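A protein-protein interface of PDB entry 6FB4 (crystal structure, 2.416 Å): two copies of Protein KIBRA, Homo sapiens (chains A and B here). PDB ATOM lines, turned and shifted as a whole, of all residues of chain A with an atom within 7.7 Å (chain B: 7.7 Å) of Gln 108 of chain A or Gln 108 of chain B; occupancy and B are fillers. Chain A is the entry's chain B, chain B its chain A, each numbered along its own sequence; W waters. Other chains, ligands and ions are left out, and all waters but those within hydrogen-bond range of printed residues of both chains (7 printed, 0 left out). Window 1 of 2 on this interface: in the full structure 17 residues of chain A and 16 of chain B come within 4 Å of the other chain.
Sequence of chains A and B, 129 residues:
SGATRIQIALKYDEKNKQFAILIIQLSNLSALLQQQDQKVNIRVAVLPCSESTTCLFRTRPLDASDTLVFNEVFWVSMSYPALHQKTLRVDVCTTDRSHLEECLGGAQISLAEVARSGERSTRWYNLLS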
ATOM      1  N   ALA A  45     -34.943  13.213 -31.501  1.00  0.00           N
ATOM      2  CA  ALA A  45     -33.979  13.305 -32.585  1.00  0.00           C
ATOM      3  C   ALA A  45     -32.596  12.922 -32.091  1.00  0.00           C
ATOM      4  O   ALA A  45     -32.147  13.406 -31.049  1.00  0.00           O
ATOM      5  CB  ALA A  45     -33.938  14.710 -33.165  1.00  0.00           C
ATOM      6  N   LEU A  47     -28.990  13.484 -33.088  1.00  0.00           N
ATOM      7  CA  LEU A  47     -28.319  14.440 -33.930  1.00  0.00           C
ATOM      8  C   LEU A  47     -26.833  14.423 -33.653  1.00  0.00           C
ATOM      9  O   LEU A  47     -26.406  14.150 -32.522  1.00  0.00           O
ATOM     10  CB  LEU A  47     -28.858  15.853 -33.700  1.00  0.00           C
ATOM     11  CG  LEU A  47     -30.343  15.949 -34.047  1.00  0.00           C
ATOM     12  CD1 LEU A  47     -30.920  17.236 -33.542  1.00  0.00           C
ATOM     13  CD2 LEU A  47     -30.528  15.848 -35.527  1.00  0.00           C
ATOM     14  N   THR A  87     -26.039  13.681 -29.952  1.00  0.00           N
ATOM     15  CA  THR A  87     -26.826  14.375 -28.954  1.00  0.00           C
ATOM     16  C   THR A  87     -28.287  14.040 -29.194  1.00  0.00           C
ATOM     17  O   THR A  87     -28.731  13.954 -30.338  1.00  0.00           O
ATOM     18  CB  THR A  87     -26.621  15.893 -29.033  1.00  0.00           C
ATOM     19  OG1 THR A  87     -25.279  16.214 -28.663  1.00  0.00           O
ATOM     20  CG2 THR A  87     -27.582  16.637 -28.115  1.00  0.00           C
ATOM     21  N   LEU A  88     -29.029  13.892 -28.109  1.00  0.00           N
ATOM     22  CA  LEU A  88     -30.443  13.570 -28.156  1.00  0.00           C
ATOM     23  C   LEU A  88     -31.262  14.841 -27.940  1.00  0.00           C
ATOM     24  O   LEU A  88     -31.106  15.523 -26.924  1.00  0.00           O
ATOM     25  CB  LEU A  88     -30.750  12.523 -27.087  1.00  0.00           C
ATOM     26  CG  LEU A  88     -32.132  11.903 -27.090  1.00  0.00           C
ATOM     27  CD1 LEU A  88     -32.332  11.101 -28.383  1.00  0.00           C
ATOM     28  CD2 LEU A  88     -32.248  11.026 -25.860  1.00  0.00           C
ATOM     29  N   ARG A  89     -32.135  15.157 -28.890  1.00  0.00           N
ATOM     30  CA  ARG A  89     -33.025  16.309 -28.795  1.00  0.00           C
ATOM     31  C   ARG A  89     -34.464  15.818 -28.666  1.00  0.00           C
ATOM     32  O   ARG A  89     -34.988  15.197 -29.592  1.00  0.00           O
ATOM     33  CB  ARG A  89     -32.878  17.199 -30.023  1.00  0.00           C
ATOM     34  CG  ARG A  89     -33.825  18.391 -30.053  1.00  0.00           C
ATOM     35  CD  ARG A  89     -33.403  19.500 -29.086  1.00  0.00           C
ATOM     36  NE  ARG A  89     -34.530  20.367 -28.721  1.00  0.00           N
ATOM     37  CZ  ARG A  89     -34.449  21.431 -27.922  1.00  0.00           C
ATOM     38  NH1 ARG A  89     -33.284  21.807 -27.382  1.00  0.00           N
ATOM     39  NH2 ARG A  89     -35.547  22.125 -27.664  1.00  0.00           N
ATOM     40  N   VAL A  90     -35.101  16.114 -27.535  1.00  0.00           N
ATOM     41  CA  VAL A  90     -36.488  15.743 -27.281  1.00  0.00           C
ATOM     42  C   VAL A  90     -37.309  17.005 -27.115  1.00  0.00           C
ATOM     43  O   VAL A  90     -36.874  17.955 -26.458  1.00  0.00           O
ATOM     44  CB  VAL A  90     -36.648  14.854 -26.028  1.00  0.00           C
ATOM     45  CG1 VAL A  90     -35.842  13.582 -26.170  1.00  0.00           C
ATOM     46  CG2 VAL A  90     -36.185  15.589 -24.823  1.00  0.00           C
ATOM     47  N   ASP A  91     -38.516  16.995 -27.677  1.00  0.00           N
ATOM     48  CA  ASP A  91     -39.423  18.127 -27.560  1.00  0.00           C
ATOM     49  C   ASP A  91     -40.835  17.658 -27.258  1.00  0.00           C
ATOM     50  O   ASP A  91     -41.284  16.614 -27.747  1.00  0.00           O
ATOM     51  CB  ASP A  91     -39.427  18.958 -28.835  1.00  0.00           C
ATOM     52  CG  ASP A  91     -38.108  19.643 -29.068  1.00  0.00           C
ATOM     53  OD1 ASP A  91     -37.863  20.691 -28.436  1.00  0.00           O
ATOM     54  OD2 ASP A  91     -37.298  19.104 -29.849  1.00  0.00           O
ATOM     55  N   GLY A 106     -38.253  21.596 -24.644  1.00  0.00           N
ATOM     56  CA  GLY A 106     -37.417  20.476 -25.009  1.00  0.00           C
ATOM     57  C   GLY A 106     -36.166  20.464 -24.173  1.00  0.00           C
ATOM     58  O   GLY A 106     -35.961  21.315 -23.312  1.00  0.00           O
ATOM     59  N   ALA A 107     -35.340  19.462 -24.440  1.00  0.00           N
ATOM     60  CA  ALA A 107     -34.102  19.233 -23.721  1.00  0.00           C
ATOM     61  C   ALA A 107     -33.086  18.670 -24.692  1.00  0.00           C
ATOM     62  O   ALA A 107     -33.435  18.076 -25.718  1.00  0.00           O
ATOM     63  CB  ALA A 107     -34.271  18.271 -22.533  1.00  0.00           C
ATOM     64  N   GLN A 108     -31.822  18.861 -24.339  1.00  0.00           N
ATOM     65  CA  GLN A 108     -30.691  18.379 -25.112  1.00  0.00           C
ATOM     66  C   GLN A 108     -29.800  17.534 -24.216  1.00  0.00           C
ATOM     67  O   GLN A 108     -29.343  18.003 -23.168  1.00  0.00           O
ATOM     68  CB  GLN A 108     -29.916  19.545 -25.696  1.00  0.00           C
ATOM     69  CG  GLN A 108     -30.064  19.623 -27.166  1.00  0.00           C
ATOM     70  CD  GLN A 108     -29.351  20.804 -27.723  1.00  0.00           C
ATOM     71  OE1 GLN A 108     -29.973  21.677 -28.363  1.00  0.00           O
ATOM     72  NE2 GLN A 108     -28.029  20.861 -27.484  1.00  0.00           N
ATOM     73  N   ILE A 109     -29.541  16.304 -24.643  1.00  0.00           N
ATOM     74  CA  ILE A 109     -28.866  15.311 -23.829  1.00  0.00           C
ATOM     75  C   ILE A 109     -27.669  14.792 -24.620  1.00  0.00           C
ATOM     76  O   ILE A 109     -27.816  13.984 -25.543  1.00  0.00           O
ATOM     77  CB  ILE A 109     -29.796  14.174 -23.428  1.00  0.00           C
ATOM     78  CG1 ILE A 109     -31.100  14.783 -22.940  1.00  0.00           C
ATOM     79  CG2 ILE A 109     -29.121  13.298 -22.376  1.00  0.00           C
ATOM     80  CD1 ILE A 109     -32.099  13.795 -22.469  1.00  0.00           C
ATOM     81  N   SER A 110     -26.488  15.261 -24.257  1.00  0.00           N
ATOM     82  CA  SER A 110     -25.259  14.715 -24.786  1.00  0.00           C
ATOM     83  C   SER A 110     -25.173  13.226 -24.500  1.00  0.00           C
ATOM     84  O   SER A 110     -25.363  12.786 -23.362  1.00  0.00           O
ATOM     85  CB  SER A 110     -24.081  15.447 -24.145  1.00  0.00           C
ATOM     86  OG  SER A 110     -22.874  14.831 -24.511  1.00  0.00           O
ATOM     87  N   LEU A 111     -24.869  12.451 -25.534  1.00  0.00           N
ATOM     88  CA  LEU A 111     -24.684  11.011 -25.391  1.00  0.00           C
ATOM     89  C   LEU A 111     -23.222  10.618 -25.216  1.00  0.00           C
ATOM     90  O   LEU A 111     -22.904   9.428 -25.236  1.00  0.00           O
ATOM     91  CB  LEU A 111     -25.287  10.300 -26.599  1.00  0.00           C
ATOM     92  CG  LEU A 111     -26.790  10.588 -26.778  1.00  0.00           C
ATOM     93  CD1 LEU A 111     -27.309   9.875 -27.983  1.00  0.00           C
ATOM     94  CD2 LEU A 111     -27.597  10.176 -25.559  1.00  0.00           C
ATOM     95  N   TYR A 125     -34.927  14.983 -16.775  1.00  0.00           N
ATOM     96  CA  TYR A 125     -34.287  16.058 -17.520  1.00  0.00           C
ATOM     97  C   TYR A 125     -35.235  17.240 -17.564  1.00  0.00           C
ATOM     98  O   TYR A 125     -36.408  17.073 -17.907  1.00  0.00           O
ATOM     99  CB  TYR A 125     -33.926  15.617 -18.947  1.00  0.00           C
ATOM    100  CG  TYR A 125     -32.944  14.475 -19.023  1.00  0.00           C
ATOM    101  CD1 TYR A 125     -33.372  13.150 -18.951  1.00  0.00           C
ATOM    102  CD2 TYR A 125     -31.589  14.713 -19.148  1.00  0.00           C
ATOM    103  CE1 TYR A 125     -32.474  12.107 -19.016  1.00  0.00           C
ATOM    104  CE2 TYR A 125     -30.685  13.678 -19.211  1.00  0.00           C
ATOM    105  CZ  TYR A 125     -31.127  12.384 -19.149  1.00  0.00           C
ATOM    106  OH  TYR A 125     -30.209  11.362 -19.214  1.00  0.00           O
ATOM    107  N   ASN A 126     -34.737  18.424 -17.197  1.00  0.00           N
ATOM    108  CA  ASN A 126     -35.547  19.635 -17.294  1.00  0.00           C
ATOM    109  C   ASN A 126     -35.781  20.005 -18.754  1.00  0.00           C
ATOM    110  O   ASN A 126     -34.947  19.756 -19.629  1.00  0.00           O
ATOM    111  CB  ASN A 126     -34.878  20.811 -16.589  1.00  0.00           C
ATOM    112  CG  ASN A 126     -34.956  20.722 -15.085  1.00  0.00           C
ATOM    113  OD1 ASN A 126     -35.868  20.126 -14.525  1.00  0.00           O
ATOM    114  ND2 ASN A 126     -33.984  21.323 -14.419  1.00  0.00           N
ATOM    115  N   LEU A 127     -36.938  20.597 -19.018  1.00  0.00           N
ATOM    116  CA  LEU A 127     -37.267  21.087 -20.346  1.00  0.00           C
ATOM    117  C   LEU A 127     -37.188  22.607 -20.346  1.00  0.00           C
ATOM    118  O   LEU A 127     -37.686  23.269 -19.425  1.00  0.00           O
ATOM    119  CB  LEU A 127     -38.659  20.632 -20.791  1.00  0.00           C
ATOM    120  CG  LEU A 127     -38.945  19.123 -20.829  1.00  0.00           C
ATOM    121  CD1 LEU A 127     -40.301  18.909 -21.411  1.00  0.00           C
ATOM    122  CD2 LEU A 127     -37.897  18.330 -21.609  1.00  0.00           C
ATOM    123  N   LEU A 128     -36.544  23.150 -21.366  1.00  0.00           N
ATOM    124  CA  LEU A 128     -36.502  24.580 -21.570  1.00  0.00           C
ATOM    125  C   LEU A 128     -37.529  25.004 -22.598  1.00  0.00           C
ATOM    126  O   LEU A 128     -37.549  24.489 -23.717  1.00  0.00           O
ATOM    127  CB  LEU A 128     -35.137  25.000 -22.043  1.00  0.00           C
ATOM    128  CG  LEU A 128     -34.200  25.576 -21.037  1.00  0.00           C
ATOM    129  CD1 LEU A 128     -32.994  26.041 -21.860  1.00  0.00           C
ATOM    130  CD2 LEU A 128     -34.831  26.730 -20.255  1.00  0.00           C
ATOM    131  N   ALA B  45     -24.631  30.170 -19.766  1.00  0.00           N
ATOM    132  CA  ALA B  45     -25.895  30.763 -19.358  1.00  0.00           C
ATOM    133  C   ALA B  45     -26.655  29.799 -18.464  1.00  0.00           C
ATOM    134  O   ALA B  45     -26.739  28.604 -18.761  1.00  0.00           O
ATOM    135  CB  ALA B  45     -26.727  31.124 -20.576  1.00  0.00           C
ATOM    136  N   LEU B  47     -30.229  28.968 -17.303  1.00  0.00           N
ATOM    137  CA  LEU B  47     -31.526  29.279 -17.852  1.00  0.00           C
ATOM    138  C   LEU B  47     -32.591  28.428 -17.188  1.00  0.00           C
ATOM    139  O   LEU B  47     -32.297  27.355 -16.661  1.00  0.00           O
ATOM    140  CB  LEU B  47     -31.559  29.041 -19.363  1.00  0.00           C
ATOM    141  CG  LEU B  47     -30.484  29.812 -20.132  1.00  0.00           C
ATOM    142  CD1 LEU B  47     -30.406  29.304 -21.549  1.00  0.00           C
ATOM    143  CD2 LEU B  47     -30.800  31.288 -20.111  1.00  0.00           C
ATOM    144  N   THR B  87     -31.408  24.883 -16.489  1.00  0.00           N
ATOM    145  CA  THR B  87     -30.584  24.250 -17.507  1.00  0.00           C
ATOM    146  C   THR B  87     -29.345  25.110 -17.751  1.00  0.00           C
ATOM    147  O   THR B  87     -29.439  26.335 -17.835  1.00  0.00           O
ATOM    148  CB  THR B  87     -31.373  24.079 -18.807  1.00  0.00           C
ATOM    149  OG1 THR B  87     -32.548  23.300 -18.558  1.00  0.00           O
ATOM    150  CG2 THR B  87     -30.546  23.392 -19.858  1.00  0.00           C
ATOM    151  N   LEU B  88     -28.182  24.467 -17.844  1.00  0.00           N
ATOM    152  CA  LEU B  88     -26.934  25.152 -18.164  1.00  0.00           C
ATOM    153  C   LEU B  88     -26.690  25.096 -19.657  1.00  0.00           C
ATOM    154  O   LEU B  88     -26.675  24.014 -20.248  1.00  0.00           O
ATOM    155  CB  LEU B  88     -25.746  24.509 -17.449  1.00  0.00           C
ATOM    156  CG  LEU B  88     -24.453  25.327 -17.541  1.00  0.00           C
ATOM    157  CD1 LEU B  88     -24.536  26.581 -16.650  1.00  0.00           C
ATOM    158  CD2 LEU B  88     -23.235  24.481 -17.176  1.00  0.00           C
ATOM    159  N   ARG B  89     -26.490  26.252 -20.267  1.00  0.00           N
ATOM    160  CA  ARG B  89     -26.185  26.317 -21.685  1.00  0.00           C
ATOM    161  C   ARG B  89     -24.769  26.847 -21.866  1.00  0.00           C
ATOM    162  O   ARG B  89     -24.430  27.914 -21.346  1.00  0.00           O
ATOM    163  CB  ARG B  89     -27.207  27.187 -22.410  1.00  0.00           C
ATOM    164  CG  ARG B  89     -26.884  27.400 -23.847  1.00  0.00           C
ATOM    165  CD  ARG B  89     -28.074  27.784 -24.676  1.00  0.00           C
ATOM    166  NE  ARG B  89     -27.602  28.336 -25.946  1.00  0.00           N
ATOM    167  CZ  ARG B  89     -28.358  28.958 -26.842  1.00  0.00           C
ATOM    168  NH1 ARG B  89     -29.659  29.110 -26.637  1.00  0.00           N
ATOM    169  NH2 ARG B  89     -27.803  29.426 -27.957  1.00  0.00           N
ATOM    170  N   VAL B  90     -23.938  26.097 -22.591  1.00  0.00           N
ATOM    171  CA  VAL B  90     -22.567  26.500 -22.872  1.00  0.00           C
ATOM    172  C   VAL B  90     -22.346  26.453 -24.378  1.00  0.00           C
ATOM    173  O   VAL B  90     -22.732  25.484 -25.040  1.00  0.00           O
ATOM    174  CB  VAL B  90     -21.538  25.625 -22.134  1.00  0.00           C
ATOM    175  CG1 VAL B  90     -21.821  25.639 -20.642  1.00  0.00           C
ATOM    176  CG2 VAL B  90     -21.577  24.236 -22.641  1.00  0.00           C
ATOM    177  N   ASP B  91     -21.728  27.503 -24.912  1.00  0.00           N
ATOM    178  CA  ASP B  91     -21.526  27.645 -26.343  1.00  0.00           C
ATOM    179  C   ASP B  91     -20.079  28.020 -26.612  1.00  0.00           C
ATOM    180  O   ASP B  91     -19.532  28.914 -25.958  1.00  0.00           O
ATOM    181  CB  ASP B  91     -22.456  28.700 -26.909  1.00  0.00           C
ATOM    182  CG  ASP B  91     -23.889  28.270 -26.859  1.00  0.00           C
ATOM    183  OD1 ASP B  91     -24.190  27.226 -27.466  1.00  0.00           O
ATOM    184  OD2 ASP B  91     -24.704  28.958 -26.205  1.00  0.00           O
ATOM    185  N   GLY B 105     -21.571  26.387 -31.694  1.00  0.00           N
ATOM    186  CA  GLY B 105     -22.189  25.178 -31.210  1.00  0.00           C
ATOM    187  C   GLY B 105     -22.147  25.175 -29.701  1.00  0.00           C
ATOM    188  O   GLY B 105     -21.440  25.968 -29.078  1.00  0.00           O
ATOM    189  N   GLY B 106     -22.922  24.269 -29.131  1.00  0.00           N
ATOM    190  CA  GLY B 106     -22.985  24.250 -27.685  1.00  0.00           C
ATOM    191  C   GLY B 106     -23.651  23.004 -27.167  1.00  0.00           C
ATOM    192  O   GLY B 106     -24.010  22.092 -27.919  1.00  0.00           O
ATOM    193  N   ALA B 107     -23.800  22.992 -25.842  1.00  0.00           N
ATOM    194  CA  ALA B 107     -24.459  21.931 -25.108  1.00  0.00           C
ATOM    195  C   ALA B 107     -25.462  22.550 -24.152  1.00  0.00           C
ATOM    196  O   ALA B 107     -25.362  23.724 -23.784  1.00  0.00           O
ATOM    197  CB  ALA B 107     -23.470  21.083 -24.313  1.00  0.00           C
ATOM    198  N   GLN B 108     -26.434  21.739 -23.763  1.00  0.00           N
ATOM    199  CA  GLN B 108     -27.394  22.091 -22.733  1.00  0.00           C
ATOM    200  C   GLN B 108     -27.448  20.957 -21.735  1.00  0.00           C
ATOM    201  O   GLN B 108     -27.445  19.771 -22.100  1.00  0.00           O
ATOM    202  CB  GLN B 108     -28.763  22.342 -23.290  1.00  0.00           C
ATOM    203  CG  GLN B 108     -28.807  23.410 -24.357  1.00  0.00           C
ATOM    204  CD  GLN B 108     -30.233  23.880 -24.652  1.00  0.00           C
ATOM    205  OE1 GLN B 108     -31.218  23.295 -24.176  1.00  0.00           O
ATOM    206  NE2 GLN B 108     -30.347  24.942 -25.437  1.00  0.00           N
ATOM    207  N   ILE B 109     -27.467  21.330 -20.468  1.00  0.00           N
ATOM    208  CA  ILE B 109     -27.298  20.381 -19.397  1.00  0.00           C
ATOM    209  C   ILE B 109     -28.382  20.661 -18.380  1.00  0.00           C
ATOM    210  O   ILE B 109     -28.330  21.673 -17.670  1.00  0.00           O
ATOM    211  CB  ILE B 109     -25.912  20.481 -18.766  1.00  0.00           C
ATOM    212  CG1 ILE B 109     -24.854  20.478 -19.875  1.00  0.00           C
ATOM    213  CG2 ILE B 109     -25.688  19.327 -17.782  1.00  0.00           C
ATOM    214  CD1 ILE B 109     -23.454  20.746 -19.375  1.00  0.00           C
ATOM    215  N   SER B 110     -29.370  19.785 -18.321  1.00  0.00           N
ATOM    216  CA  SER B 110     -30.337  19.838 -17.248  1.00  0.00           C
ATOM    217  C   SER B 110     -29.611  19.730 -15.912  1.00  0.00           C
ATOM    218  O   SER B 110     -28.759  18.857 -15.739  1.00  0.00           O
ATOM    219  CB  SER B 110     -31.341  18.700 -17.423  1.00  0.00           C
ATOM    220  OG  SER B 110     -32.186  18.564 -16.286  1.00  0.00           O
ATOM    221  N   LEU B 111     -29.928  20.632 -14.976  1.00  0.00           N
ATOM    222  CA  LEU B 111     -29.351  20.614 -13.635  1.00  0.00           C
ATOM    223  C   LEU B 111     -30.268  19.951 -12.617  1.00  0.00           C
ATOM    224  O   LEU B 111     -30.098  20.153 -11.409  1.00  0.00           O
ATOM    225  CB  LEU B 111     -29.018  22.031 -13.174  1.00  0.00           C
ATOM    226  CG  LEU B 111     -28.197  22.854 -14.150  1.00  0.00           C
ATOM    227  CD1 LEU B 111     -27.937  24.270 -13.615  1.00  0.00           C
ATOM    228  CD2 LEU B 111     -26.903  22.147 -14.458  1.00  0.00           C
ATOM    229  N   TYR B 125     -19.210  16.663 -22.527  1.00  0.00           N
ATOM    230  CA  TYR B 125     -20.468  16.937 -23.198  1.00  0.00           C
ATOM    231  C   TYR B 125     -20.210  17.214 -24.673  1.00  0.00           C
ATOM    232  O   TYR B 125     -19.336  18.013 -25.018  1.00  0.00           O
ATOM    233  CB  TYR B 125     -21.193  18.118 -22.551  1.00  0.00           C
ATOM    234  CG  TYR B 125     -21.482  17.925 -21.079  1.00  0.00           C
ATOM    235  CD1 TYR B 125     -20.555  18.291 -20.105  1.00  0.00           C
ATOM    236  CD2 TYR B 125     -22.680  17.372 -20.662  1.00  0.00           C
ATOM    237  CE1 TYR B 125     -20.818  18.102 -18.757  1.00  0.00           C
ATOM    238  CE2 TYR B 125     -22.953  17.179 -19.325  1.00  0.00           C
ATOM    239  CZ  TYR B 125     -22.023  17.545 -18.378  1.00  0.00           C
ATOM    240  OH  TYR B 125     -22.319  17.355 -17.052  1.00  0.00           O
ATOM    241  N   ASN B 126     -20.964  16.542 -25.538  1.00  0.00           N
ATOM    242  CA  ASN B 126     -20.876  16.802 -26.958  1.00  0.00           C
ATOM    243  C   ASN B 126     -21.467  18.163 -27.266  1.00  0.00           C
ATOM    244  O   ASN B 126     -22.448  18.595 -26.655  1.00  0.00           O
ATOM    245  CB  ASN B 126     -21.596  15.718 -27.746  1.00  0.00           C
ATOM    246  CG  ASN B 126     -20.823  14.419 -27.768  1.00  0.00           C
ATOM    247  OD1 ASN B 126     -19.596  14.432 -27.702  1.00  0.00           O
ATOM    248  ND2 ASN B 126     -21.528  13.288 -27.843  1.00  0.00           N
ATOM    249  N   LEU B 127     -20.840  18.856 -28.199  1.00  0.00           N
ATOM    250  CA  LEU B 127     -21.390  20.093 -28.709  1.00  0.00           C
ATOM    251  C   LEU B 127     -22.231  19.795 -29.940  1.00  0.00           C
ATOM    252  O   LEU B 127     -21.874  18.956 -30.773  1.00  0.00           O
ATOM    253  CB  LEU B 127     -20.272  21.077 -29.048  1.00  0.00           C
ATOM    254  CG  LEU B 127     -19.347  21.444 -27.892  1.00  0.00           C
ATOM    255  CD1 LEU B 127     -18.441  22.525 -28.330  1.00  0.00           C
ATOM    256  CD2 LEU B 127     -20.117  21.913 -26.680  1.00  0.00           C
ATOM    257  N   LEU B 128     -23.360  20.471 -30.035  1.00  0.00           N
ATOM    258  CA  LEU B 128     -24.213  20.401 -31.203  1.00  0.00           C
ATOM    259  C   LEU B 128     -24.257  21.784 -31.831  1.00  0.00           C
ATOM    260  O   LEU B 128     -24.194  22.789 -31.122  1.00  0.00           O
ATOM    261  CB  LEU B 128     -25.606  19.937 -30.808  1.00  0.00           C
ATOM    262  CG  LEU B 128     -26.594  19.586 -31.903  1.00  0.00           C
ATOM    263  CD1 LEU B 128     -26.126  18.367 -32.695  1.00  0.00           C
ATOM    264  CD2 LEU B 128     -27.916  19.326 -31.242  1.00  0.00           C
ATOM    265  N   SER B 129     -24.338  21.843 -33.153  1.00  0.00           N
ATOM    266  CA  SER B 129     -24.506  23.127 -33.827  1.00  0.00           C
ATOM    267  C   SER B 129     -25.968  23.612 -33.824  1.00  0.00           C
ATOM    268  O   SER B 129     -26.919  22.831 -33.937  1.00  0.00           O
ATOM    269  CB  SER B 129     -24.004  23.033 -35.255  1.00  0.00           C
ATOM    270  OG  SER B 129     -24.579  24.054 -36.039  1.00  0.00           O
ATOM    271  OXT SER B 129     -26.237  24.815 -33.711  1.00  0.00           O
HETATM  272  O   HOH W   1     -24.837  18.140 -26.929  1.00  0.00           O
HETATM  273  O   HOH W   2     -26.419  19.130 -24.908  1.00  0.00           O
HETATM  274  O   HOH W   3     -26.412  16.942 -21.897  1.00  0.00           O
HETATM  275  O   HOH W   4     -29.088  17.504 -20.074  1.00  0.00           O
HETATM  276  O   HOH W   5     -32.730  20.980 -19.907  1.00  0.00           O
HETATM  277  O   HOH W   6     -31.441  20.651 -22.249  1.00  0.00           O
HETATM  278  O   HOH W   7     -23.609  15.936 -30.630  1.00  0.00           O
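The backbone NH (N) of Asn 126 of chain A sits at hydrogen-bond distance from the side-chain hydroxyl (OG) of Ser 110 of chain B (2.7 Å).
The backbone NH (N) of Asn 126 of chain B sits at hydrogen-bond distance from the side-chain hydroxyl (OG) of Ser 110 of chain A (2.8 Å).
The backbone carbonyl oxygen (O) of Gln 108 of chain A lies close to the backbone carbonyl oxygen (O) of Gln 108 of chain B, at 2.8 Å.
The backbone carbonyl oxygen (O) of Gly 106 of chain B is in hydrogen-bond range of the backbone NH (N) of Leu 128 of chain B, 2.7 Å away.
O of Gly 106 of chain A sits at hydrogen-bond distance from N of Leu 128 of chain A, 2.7 Å away.
The side-chain amide oxygen of Gln 108 of chain A is in hydrogen-bond range of the guanidinium group of Arg 89 of chain A, 3.5 Å away.
The backbone NH of Thr 87 of chain B sits at hydrogen-bond distance from the backbone carbonyl oxygen of Leu 47 of chain B (2.6 Å).
The backbone NH (N) of Thr 87 of chain A sits at hydrogen-bond distance from the backbone carbonyl oxygen (O) of Leu 47 of chain A (2.6 Å).
Leu 47 of chain A touches Leu 128 of chain B (CB to CD1, 3.8 Å).
Thr 87 of chain A touches Asn 126 of chain B.
CA of Tyr 125 of chain B touches OG of Ser 110 of chain A (3.5 Å).
Tyr 125 of chain A touches Ser 110 of chain B (CA to OG, 3.5 Å).
CB of Asn 126 of chain A touches OG1 of Thr 87 of chain B (3.9 Å).
Leu 128 of chain A touches Thr 87 of chain B.
Ala 107 of chain A touches none of the printed residues of chain B.
Gln 108 of chain A touches just one residue of chain B: Gln 108 (2.8 Å).
Printed residues of chain B within 4 Å of Leu 128 of chain A: Thr 87.
Of the printed residues of chain A, Thr 87 of chain B touches Asn 126 and Leu 128.
No residue of chain A comes within 4 Å of Ala 107 of chain B.
Printed residues of chain A within 4 Å of Gln 108 of chain B: Gln 108 (2.8 Å).
Of the printed residues of chain A, Ser 110 of chain B touches Tyr 125 (3.5 Å) and Asn 126 (2.7 Å).
Leu 127 of chain B touches none of the printed residues of chain A.
Of the printed residues of chain A, Leu 128 of chain B touches Leu 47.
The nearest residue of chain B that does not touch Gln 108 of chain A is Leu 128 of chain B (4.1 Å).
The nearest printed residue of chain A that does not touch Gln 108 of chain B is Leu 128 of chain A (4.01 Å).
Of the 17 printed residues of chain A, 7 touch a printed residue of chain B.
Printed residues of chain A that touch a printed residue of chain B: Leu 47, Thr 87, Gln 108, Ser 110, Tyr 125, Asn 126 and Leu 128.
Along chain A the printed residues that touch a printed residue of chain B span positions 47 to 128.
Along chain B the printed residues that touch a printed residue of chain A span positions 87 to 128.
Among the printed residues, no Asp or Glu carboxylate lies within 4 Å of a Lys or Arg side-chain nitrogen of the other chain.
Thr 87 of chain A touches Asn 126 of chain B, and with the chains exchanged Asn 126 of chain A touches Thr 87 of chain B.
Gln 108 of chain A touches its own counterpart, Gln 108 of chain B.
Ser 110 of chain A touches Tyr 125 of chain B, and with the chains exchanged Tyr 125 of chain A touches Ser 110 of chain B.
Leu 128 of chain A touches Thr 87 of chain B, but with the chains exchanged Thr 87 of chain A does not touch Leu 128 of chain B (4.1 Å).
17 positions are printed for both chains.
Water W1 bridges O of Asn 126 of chain B (2.4 Å) and OG1 of Thr 87 of chain A (2.6 Å).
Water W5 lies within hydrogen-bond range of O of Asn 126 of chain A and OG1 of Thr 87 of chain B.
Water W6 bridges N of Gln 108 of chain A (2.8 Å) and OE1 of Gln 108 of chain B (3.3 Å).
Water W2 bridges the backbone NH (N) of Gln 108 of chain B (2.8 Å) and the side-chain amide nitrogen (NE2) of Gln 108 of chain A (3.5 Å).
Water W4 lies within hydrogen-bond range of N of Ser 110 of chain B (2.9 Å), O of Gln 108 of chain A (3.1 Å) and O of Gln 108 of chain B (3.5 Å).
Water W3 lies within hydrogen-bond range of N of Ser 110 of chain A (2.9 Å), O of Gln 108 of chain B (3.0 Å) and O of Gln 108 of chain A (3.4 Å).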
